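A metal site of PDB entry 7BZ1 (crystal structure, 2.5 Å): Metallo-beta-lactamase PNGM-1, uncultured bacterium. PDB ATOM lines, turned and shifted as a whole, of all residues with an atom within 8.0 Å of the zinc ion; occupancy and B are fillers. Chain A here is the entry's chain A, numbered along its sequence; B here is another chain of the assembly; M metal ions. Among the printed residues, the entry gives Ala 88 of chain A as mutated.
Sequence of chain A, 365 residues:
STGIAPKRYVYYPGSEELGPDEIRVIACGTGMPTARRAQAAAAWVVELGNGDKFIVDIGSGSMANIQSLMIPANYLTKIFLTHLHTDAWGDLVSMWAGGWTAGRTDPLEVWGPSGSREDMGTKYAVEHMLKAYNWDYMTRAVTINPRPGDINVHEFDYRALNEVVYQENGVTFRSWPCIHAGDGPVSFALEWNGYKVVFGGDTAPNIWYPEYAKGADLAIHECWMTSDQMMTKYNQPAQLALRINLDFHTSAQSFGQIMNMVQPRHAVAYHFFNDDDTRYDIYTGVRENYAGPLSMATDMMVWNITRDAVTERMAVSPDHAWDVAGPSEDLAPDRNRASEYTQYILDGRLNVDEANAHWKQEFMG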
ATOM      1  N   PRO A  33     -17.301 -25.750 -27.414  1.00  0.00           N
ATOM      2  CA  PRO A  33     -18.297 -25.808 -28.486  1.00  0.00           C
ATOM      3  C   PRO A  33     -18.099 -26.935 -29.524  1.00  0.00           C
ATOM      4  O   PRO A  33     -19.022 -27.199 -30.284  1.00  0.00           O
ATOM      5  CB  PRO A  33     -18.257 -24.423 -29.170  1.00  0.00           C
ATOM      6  CG  PRO A  33     -17.047 -23.706 -28.568  1.00  0.00           C
ATOM      7  CD  PRO A  33     -16.693 -24.411 -27.279  1.00  0.00           C
ATOM      8  N   ALA A  42     -20.806 -27.691 -21.272  1.00  0.00           N
ATOM      9  CA  ALA A  42     -20.970 -27.403 -19.826  1.00  0.00           C
ATOM     10  C   ALA A  42     -22.262 -27.983 -19.227  1.00  0.00           C
ATOM     11  O   ALA A  42     -23.363 -27.715 -19.748  1.00  0.00           O
ATOM     12  CB  ALA A  42     -20.901 -25.912 -19.610  1.00  0.00           C
ATOM     13  N   ASP A  57     -26.391 -25.167 -16.069  1.00  0.00           N
ATOM     14  CA  ASP A  57     -25.971 -25.351 -17.492  1.00  0.00           C
ATOM     15  C   ASP A  57     -26.330 -26.787 -17.914  1.00  0.00           C
ATOM     16  O   ASP A  57     -26.178 -27.715 -17.123  1.00  0.00           O
ATOM     17  CB  ASP A  57     -24.513 -24.924 -17.744  1.00  0.00           C
ATOM     18  CG  ASP A  57     -24.295 -23.418 -17.837  1.00  0.00           C
ATOM     19  OD1 ASP A  57     -25.330 -22.702 -17.815  1.00  0.00           O
ATOM     20  OD2 ASP A  57     -23.111 -22.953 -17.969  1.00  0.00           O
ATOM     21  N   THR A  82     -26.341 -20.220 -17.282  1.00  0.00           N
ATOM     22  CA  THR A  82     -25.385 -19.082 -17.150  1.00  0.00           C
ATOM     23  C   THR A  82     -25.541 -18.166 -18.348  1.00  0.00           C
ATOM     24  O   THR A  82     -25.408 -16.951 -18.127  1.00  0.00           O
ATOM     25  CB  THR A  82     -23.943 -19.538 -16.968  1.00  0.00           C
ATOM     26  OG1 THR A  82     -23.574 -20.261 -18.139  1.00  0.00           O
ATOM     27  CG2 THR A  82     -23.751 -20.319 -15.686  1.00  0.00           C
ATOM     28  N   HIS A  83     -25.865 -18.710 -19.534  1.00  0.00           N
ATOM     29  CA  HIS A  83     -25.957 -17.949 -20.811  1.00  0.00           C
ATOM     30  C   HIS A  83     -26.548 -18.821 -21.937  1.00  0.00           C
ATOM     31  O   HIS A  83     -26.744 -19.977 -21.758  1.00  0.00           O
ATOM     32  CB  HIS A  83     -24.586 -17.344 -21.181  1.00  0.00           C
ATOM     33  CG  HIS A  83     -23.500 -18.316 -21.511  1.00  0.00           C
ATOM     34  ND1 HIS A  83     -22.928 -19.132 -20.566  1.00  0.00           N
ATOM     35  CD2 HIS A  83     -22.833 -18.554 -22.654  1.00  0.00           C
ATOM     36  CE1 HIS A  83     -21.940 -19.814 -21.116  1.00  0.00           C
ATOM     37  NE2 HIS A  83     -21.859 -19.473 -22.384  1.00  0.00           N
ATOM     38  N   LEU A  84     -26.825 -18.224 -23.070  1.00  0.00           N
ATOM     39  CA  LEU A  84     -27.651 -18.876 -24.119  1.00  0.00           C
ATOM     40  C   LEU A  84     -26.808 -19.345 -25.295  1.00  0.00           C
ATOM     41  O   LEU A  84     -27.317 -19.256 -26.410  1.00  0.00           O
ATOM     42  CB  LEU A  84     -28.694 -17.869 -24.603  1.00  0.00           C
ATOM     43  CG  LEU A  84     -29.561 -17.328 -23.469  1.00  0.00           C
ATOM     44  CD1 LEU A  84     -30.383 -16.139 -23.960  1.00  0.00           C
ATOM     45  CD2 LEU A  84     -30.406 -18.471 -22.925  1.00  0.00           C
ATOM     46  N   HIS A  85     -25.565 -19.750 -25.041  1.00  0.00           N
ATOM     47  CA  HIS A  85     -24.736 -20.486 -26.038  1.00  0.00           C
ATOM     48  C   HIS A  85     -25.297 -21.904 -26.159  1.00  0.00           C
ATOM     49  O   HIS A  85     -25.785 -22.411 -25.111  1.00  0.00           O
ATOM     50  CB  HIS A  85     -23.248 -20.533 -25.624  1.00  0.00           C
ATOM     51  CG  HIS A  85     -22.422 -19.432 -26.196  1.00  0.00           C
ATOM     52  ND1 HIS A  85     -21.316 -18.966 -25.559  1.00  0.00           N
ATOM     53  CD2 HIS A  85     -22.496 -18.763 -27.364  1.00  0.00           C
ATOM     54  CE1 HIS A  85     -20.747 -18.021 -26.301  1.00  0.00           C
ATOM     55  NE2 HIS A  85     -21.455 -17.867 -27.395  1.00  0.00           N
ATOM     56  N   THR A  86     -25.229 -22.477 -27.382  1.00  0.00           N
ATOM     57  CA  THR A  86     -25.614 -23.884 -27.706  1.00  0.00           C
ATOM     58  C   THR A  86     -24.941 -24.759 -26.670  1.00  0.00           C
ATOM     59  O   THR A  86     -25.615 -25.555 -26.069  1.00  0.00           O
ATOM     60  CB  THR A  86     -25.241 -24.321 -29.140  1.00  0.00           C
ATOM     61  OG1 THR A  86     -23.844 -24.147 -29.356  1.00  0.00           O
ATOM     62  CG2 THR A  86     -25.921 -23.545 -30.240  1.00  0.00           C
ATOM     63  N   ASP A  87     -23.682 -24.500 -26.392  1.00  0.00           N
ATOM     64  CA  ASP A  87     -22.844 -25.347 -25.513  1.00  0.00           C
ATOM     65  C   ASP A  87     -23.098 -25.019 -24.018  1.00  0.00           C
ATOM     66  O   ASP A  87     -22.372 -25.525 -23.184  1.00  0.00           O
ATOM     67  CB  ASP A  87     -21.389 -25.278 -26.001  1.00  0.00           C
ATOM     68  CG  ASP A  87     -20.569 -24.063 -25.596  1.00  0.00           C
ATOM     69  OD1 ASP A  87     -21.073 -22.921 -25.739  1.00  0.00           O
ATOM     70  OD2 ASP A  87     -19.395 -24.278 -25.156  1.00  0.00           O
ATOM     71  N   ALA A  88     -24.122 -24.233 -23.667  1.00  0.00           N
ATOM     72  CA  ALA A  88     -24.553 -24.058 -22.262  1.00  0.00           C
ATOM     73  C   ALA A  88     -26.023 -24.442 -22.055  1.00  0.00           C
ATOM     74  O   ALA A  88     -26.396 -24.479 -20.910  1.00  0.00           O
ATOM     75  CB  ALA A  88     -24.339 -22.643 -21.805  1.00  0.00           C
ATOM     76  N   HIS A 180     -18.417 -12.011 -22.000  1.00  0.00           N
ATOM     77  CA  HIS A 180     -18.499 -13.253 -22.800  1.00  0.00           C
ATOM     78  C   HIS A 180     -19.419 -13.057 -24.014  1.00  0.00           C
ATOM     79  O   HIS A 180     -20.666 -13.113 -23.837  1.00  0.00           O
ATOM     80  CB  HIS A 180     -18.886 -14.454 -21.911  1.00  0.00           C
ATOM     81  CG  HIS A 180     -18.927 -15.740 -22.668  1.00  0.00           C
ATOM     82  ND1 HIS A 180     -17.864 -16.181 -23.461  1.00  0.00           N
ATOM     83  CD2 HIS A 180     -19.917 -16.642 -22.819  1.00  0.00           C
ATOM     84  CE1 HIS A 180     -18.201 -17.304 -24.047  1.00  0.00           C
ATOM     85  NE2 HIS A 180     -19.461 -17.626 -23.668  1.00  0.00           N
ATOM     86  N   ALA A 181     -18.822 -12.824 -25.194  1.00  0.00           N
ATOM     87  CA  ALA A 181     -19.487 -12.682 -26.517  1.00  0.00           C
ATOM     88  C   ALA A 181     -20.323 -11.380 -26.599  1.00  0.00           C
ATOM     89  O   ALA A 181     -20.257 -10.710 -27.635  1.00  0.00           O
ATOM     90  CB  ALA A 181     -20.308 -13.926 -26.801  1.00  0.00           C
ATOM     91  N   PRO A 185     -24.633 -12.989 -20.333  1.00  0.00           N
ATOM     92  CA  PRO A 185     -23.988 -14.017 -19.524  1.00  0.00           C
ATOM     93  C   PRO A 185     -23.786 -13.609 -18.068  1.00  0.00           C
ATOM     94  O   PRO A 185     -23.436 -12.471 -17.833  1.00  0.00           O
ATOM     95  CB  PRO A 185     -22.673 -14.252 -20.265  1.00  0.00           C
ATOM     96  CG  PRO A 185     -23.026 -13.956 -21.716  1.00  0.00           C
ATOM     97  CD  PRO A 185     -23.989 -12.793 -21.639  1.00  0.00           C
ATOM     98  N   GLY A 201     -19.791 -20.069 -15.057  1.00  0.00           N
ATOM     99  CA  GLY A 201     -20.113 -19.998 -16.499  1.00  0.00           C
ATOM    100  C   GLY A 201     -18.876 -19.622 -17.326  1.00  0.00           C
ATOM    101  O   GLY A 201     -17.762 -20.207 -17.078  1.00  0.00           O
ATOM    102  N   ASP A 202     -19.043 -18.719 -18.281  1.00  0.00           N
ATOM    103  CA  ASP A 202     -18.059 -18.415 -19.361  1.00  0.00           C
ATOM    104  C   ASP A 202     -17.784 -16.927 -19.299  1.00  0.00           C
ATOM    105  O   ASP A 202     -18.777 -16.163 -19.196  1.00  0.00           O
ATOM    106  CB  ASP A 202     -18.584 -18.734 -20.763  1.00  0.00           C
ATOM    107  CG  ASP A 202     -18.793 -20.214 -21.031  1.00  0.00           C
ATOM    108  OD1 ASP A 202     -18.679 -20.952 -20.056  1.00  0.00           O
ATOM    109  OD2 ASP A 202     -19.090 -20.616 -22.200  1.00  0.00           O
ATOM    110  N   THR A 203     -16.510 -16.532 -19.282  1.00  0.00           N
ATOM    111  CA  THR A 203     -16.097 -15.140 -18.986  1.00  0.00           C
ATOM    112  C   THR A 203     -14.590 -14.950 -19.194  1.00  0.00           C
ATOM    113  O   THR A 203     -13.794 -15.840 -18.809  1.00  0.00           O
ATOM    114  CB  THR A 203     -16.477 -14.696 -17.574  1.00  0.00           C
ATOM    115  OG1 THR A 203     -16.418 -13.265 -17.476  1.00  0.00           O
ATOM    116  CG2 THR A 203     -15.607 -15.332 -16.515  1.00  0.00           C
ATOM    117  N   GLU A 222     -14.110 -20.805 -15.857  1.00  0.00           N
ATOM    118  CA  GLU A 222     -13.478 -20.978 -17.188  1.00  0.00           C
ATOM    119  C   GLU A 222     -11.972 -20.900 -16.993  1.00  0.00           C
ATOM    120  O   GLU A 222     -11.540 -20.097 -16.166  1.00  0.00           O
ATOM    121  CB  GLU A 222     -13.921 -19.851 -18.100  1.00  0.00           C
ATOM    122  CG  GLU A 222     -13.494 -20.003 -19.532  1.00  0.00           C
ATOM    123  CD  GLU A 222     -13.891 -18.784 -20.360  1.00  0.00           C
ATOM    124  OE1 GLU A 222     -15.102 -18.473 -20.424  1.00  0.00           O
ATOM    125  OE2 GLU A 222     -12.980 -18.140 -20.918  1.00  0.00           O
ATOM    126  N   TRP A 224      -8.812 -21.458 -19.910  1.00  0.00           N
ATOM    127  CA  TRP A 224      -8.731 -21.725 -21.367  1.00  0.00           C
ATOM    128  C   TRP A 224      -7.433 -22.432 -21.716  1.00  0.00           C
ATOM    129  O   TRP A 224      -6.508 -22.432 -20.912  1.00  0.00           O
ATOM    130  CB  TRP A 224      -8.888 -20.456 -22.190  1.00  0.00           C
ATOM    131  CG  TRP A 224      -9.557 -20.703 -23.497  1.00  0.00           C
ATOM    132  CD1 TRP A 224      -8.963 -20.764 -24.730  1.00  0.00           C
ATOM    133  CD2 TRP A 224     -10.946 -20.957 -23.705  1.00  0.00           C
ATOM    134  NE1 TRP A 224      -9.905 -21.029 -25.683  1.00  0.00           N
ATOM    135  CE2 TRP A 224     -11.129 -21.163 -25.097  1.00  0.00           C
ATOM    136  CE3 TRP A 224     -12.049 -21.057 -22.853  1.00  0.00           C
ATOM    137  CZ2 TRP A 224     -12.379 -21.410 -25.662  1.00  0.00           C
ATOM    138  CZ3 TRP A 224     -13.286 -21.305 -23.415  1.00  0.00           C
ATOM    139  CH2 TRP A 224     -13.444 -21.477 -24.799  1.00  0.00           C
ATOM    140  N   HIS A 249     -11.252 -14.960 -23.485  1.00  0.00           N
ATOM    141  CA  HIS A 249     -11.315 -16.013 -22.429  1.00  0.00           C
ATOM    142  C   HIS A 249     -10.326 -15.763 -21.281  1.00  0.00           C
ATOM    143  O   HIS A 249      -9.433 -14.941 -21.446  1.00  0.00           O
ATOM    144  CB  HIS A 249     -11.060 -17.388 -23.063  1.00  0.00           C
ATOM    145  CG  HIS A 249     -12.001 -17.716 -24.175  1.00  0.00           C
ATOM    146  ND1 HIS A 249     -13.355 -17.985 -23.941  1.00  0.00           N
ATOM    147  CD2 HIS A 249     -11.819 -17.764 -25.513  1.00  0.00           C
ATOM    148  CE1 HIS A 249     -13.940 -18.214 -25.096  1.00  0.00           C
ATOM    149  NE2 HIS A 249     -13.024 -18.090 -26.087  1.00  0.00           N
ATOM    150  N   TYR A 270     -12.209 -25.615 -15.576  1.00  0.00           N
ATOM    151  CA  TYR A 270     -13.003 -26.374 -16.570  1.00  0.00           C
ATOM    152  C   TYR A 270     -12.991 -25.575 -17.858  1.00  0.00           C
ATOM    153  O   TYR A 270     -12.571 -24.426 -17.816  1.00  0.00           O
ATOM    154  CB  TYR A 270     -14.420 -26.650 -16.011  1.00  0.00           C
ATOM    155  CG  TYR A 270     -15.493 -25.644 -16.363  1.00  0.00           C
ATOM    156  CD1 TYR A 270     -15.529 -24.396 -15.793  1.00  0.00           C
ATOM    157  CD2 TYR A 270     -16.481 -25.963 -17.279  1.00  0.00           C
ATOM    158  CE1 TYR A 270     -16.507 -23.465 -16.148  1.00  0.00           C
ATOM    159  CE2 TYR A 270     -17.469 -25.055 -17.633  1.00  0.00           C
ATOM    160  CZ  TYR A 270     -17.498 -23.800 -17.060  1.00  0.00           C
ATOM    161  OH  TYR A 270     -18.512 -22.915 -17.384  1.00  0.00           O
ATOM    162  N   HIS A 271     -13.480 -26.186 -18.930  1.00  0.00           N
ATOM    163  CA  HIS A 271     -13.815 -25.544 -20.232  1.00  0.00           C
ATOM    164  C   HIS A 271     -12.582 -25.529 -21.133  1.00  0.00           C
ATOM    165  O   HIS A 271     -12.500 -24.688 -22.027  1.00  0.00           O
ATOM    166  CB  HIS A 271     -14.429 -24.158 -19.969  1.00  0.00           C
ATOM    167  CG  HIS A 271     -15.492 -23.812 -20.956  1.00  0.00           C
ATOM    168  ND1 HIS A 271     -15.207 -23.623 -22.302  1.00  0.00           N
ATOM    169  CD2 HIS A 271     -16.817 -23.616 -20.796  1.00  0.00           C
ATOM    170  CE1 HIS A 271     -16.324 -23.314 -22.936  1.00  0.00           C
ATOM    171  NE2 HIS A 271     -17.325 -23.286 -22.025  1.00  0.00           N
ATOM    172  N   TRP B 135     -29.387 -15.127 -29.358  1.00  0.00           N
ATOM    173  CA  TRP B 135     -28.248 -14.514 -28.624  1.00  0.00           C
ATOM    174  C   TRP B 135     -26.941 -15.077 -29.180  1.00  0.00           C
ATOM    175  O   TRP B 135     -26.122 -14.263 -29.609  1.00  0.00           O
ATOM    176  CB  TRP B 135     -28.361 -14.674 -27.117  1.00  0.00           C
ATOM    177  CG  TRP B 135     -27.284 -13.956 -26.383  1.00  0.00           C
ATOM    178  CD1 TRP B 135     -27.297 -12.687 -25.909  1.00  0.00           C
ATOM    179  CD2 TRP B 135     -26.001 -14.501 -26.037  1.00  0.00           C
ATOM    180  NE1 TRP B 135     -26.104 -12.397 -25.284  1.00  0.00           N
ATOM    181  CE2 TRP B 135     -25.296 -13.496 -25.337  1.00  0.00           C
ATOM    182  CE3 TRP B 135     -25.373 -15.728 -26.261  1.00  0.00           C
ATOM    183  CZ2 TRP B 135     -24.003 -13.688 -24.864  1.00  0.00           C
ATOM    184  CZ3 TRP B 135     -24.095 -15.921 -25.760  1.00  0.00           C
ATOM    185  CH2 TRP B 135     -23.418 -14.914 -25.090  1.00  0.00           C
ATOM    186  N   ASP B 136     -26.777 -16.395 -29.184  1.00  0.00           N
ATOM    187  CA  ASP B 136     -25.641 -17.119 -29.830  1.00  0.00           C
ATOM    188  C   ASP B 136     -25.384 -16.451 -31.198  1.00  0.00           C
ATOM    189  O   ASP B 136     -24.247 -16.052 -31.451  1.00  0.00           O
ATOM    190  CB  ASP B 136     -25.900 -18.631 -29.959  1.00  0.00           C
ATOM    191  CG  ASP B 136     -24.667 -19.461 -30.333  1.00  0.00           C
ATOM    192  OD1 ASP B 136     -24.042 -19.166 -31.377  1.00  0.00           O
ATOM    193  OD2 ASP B 136     -24.305 -20.391 -29.553  1.00  0.00           O
ATOM    194  N   ARG B 140     -22.029 -14.026 -32.033  1.00  0.00           N
ATOM    195  CA  ARG B 140     -21.164 -14.690 -33.051  1.00  0.00           C
ATOM    196  C   ARG B 140     -21.010 -13.768 -34.269  1.00  0.00           C
ATOM    197  O   ARG B 140     -19.860 -13.502 -34.699  1.00  0.00           O
ATOM    198  CB  ARG B 140     -21.768 -16.062 -33.369  1.00  0.00           C
ATOM    199  CG  ARG B 140     -20.900 -16.993 -34.214  1.00  0.00           C
ATOM    200  CD  ARG B 140     -21.253 -18.472 -34.026  1.00  0.00           C
ATOM    201  NE  ARG B 140     -21.034 -18.858 -32.632  1.00  0.00           N
ATOM    202  CZ  ARG B 140     -20.891 -20.094 -32.141  1.00  0.00           C
ATOM    203  NH1 ARG B 140     -20.947 -21.154 -32.935  1.00  0.00           N
ATOM    204  NH2 ARG B 140     -20.694 -20.259 -30.842  1.00  0.00           N
HETATM  205 ZN    ZN M   1     -20.270 -19.591 -23.864  1.00  0.00          ZN
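Asp 87 touches the zinc ion (OD1 to ZN, 3.9 Å). Five residues have an atom within 4 Å of the zinc ion: His 83, His 85, Asp 87, His 180 and Asp 202. The nearest printed residue that does not touch the zinc ion is His 271 (5.1 Å).
The zinc ion is bound by a ring nitrogen (ND1) of His 85, a ring nitrogen (NE2) of His 180, a ring nitrogen (NE2) of His 83 and the side-chain carboxylate (OD2) of Asp 202.
A ring nitrogen (ND1) of His 83 lies within hydrogen-bond range of the side-chain hydroxyl of Thr 82, 2.8 Å away. The side-chain carboxylate of Asp 202 sits close to a ring nitrogen (NE2) of His 271 (3.3 Å). OH of Tyr 270 lies within hydrogen-bond range of OD1 of Asp 202, 3.3 Å away. O of Asp 87 is in hydrogen-bond range of N of Ala 42 (3.3 Å).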
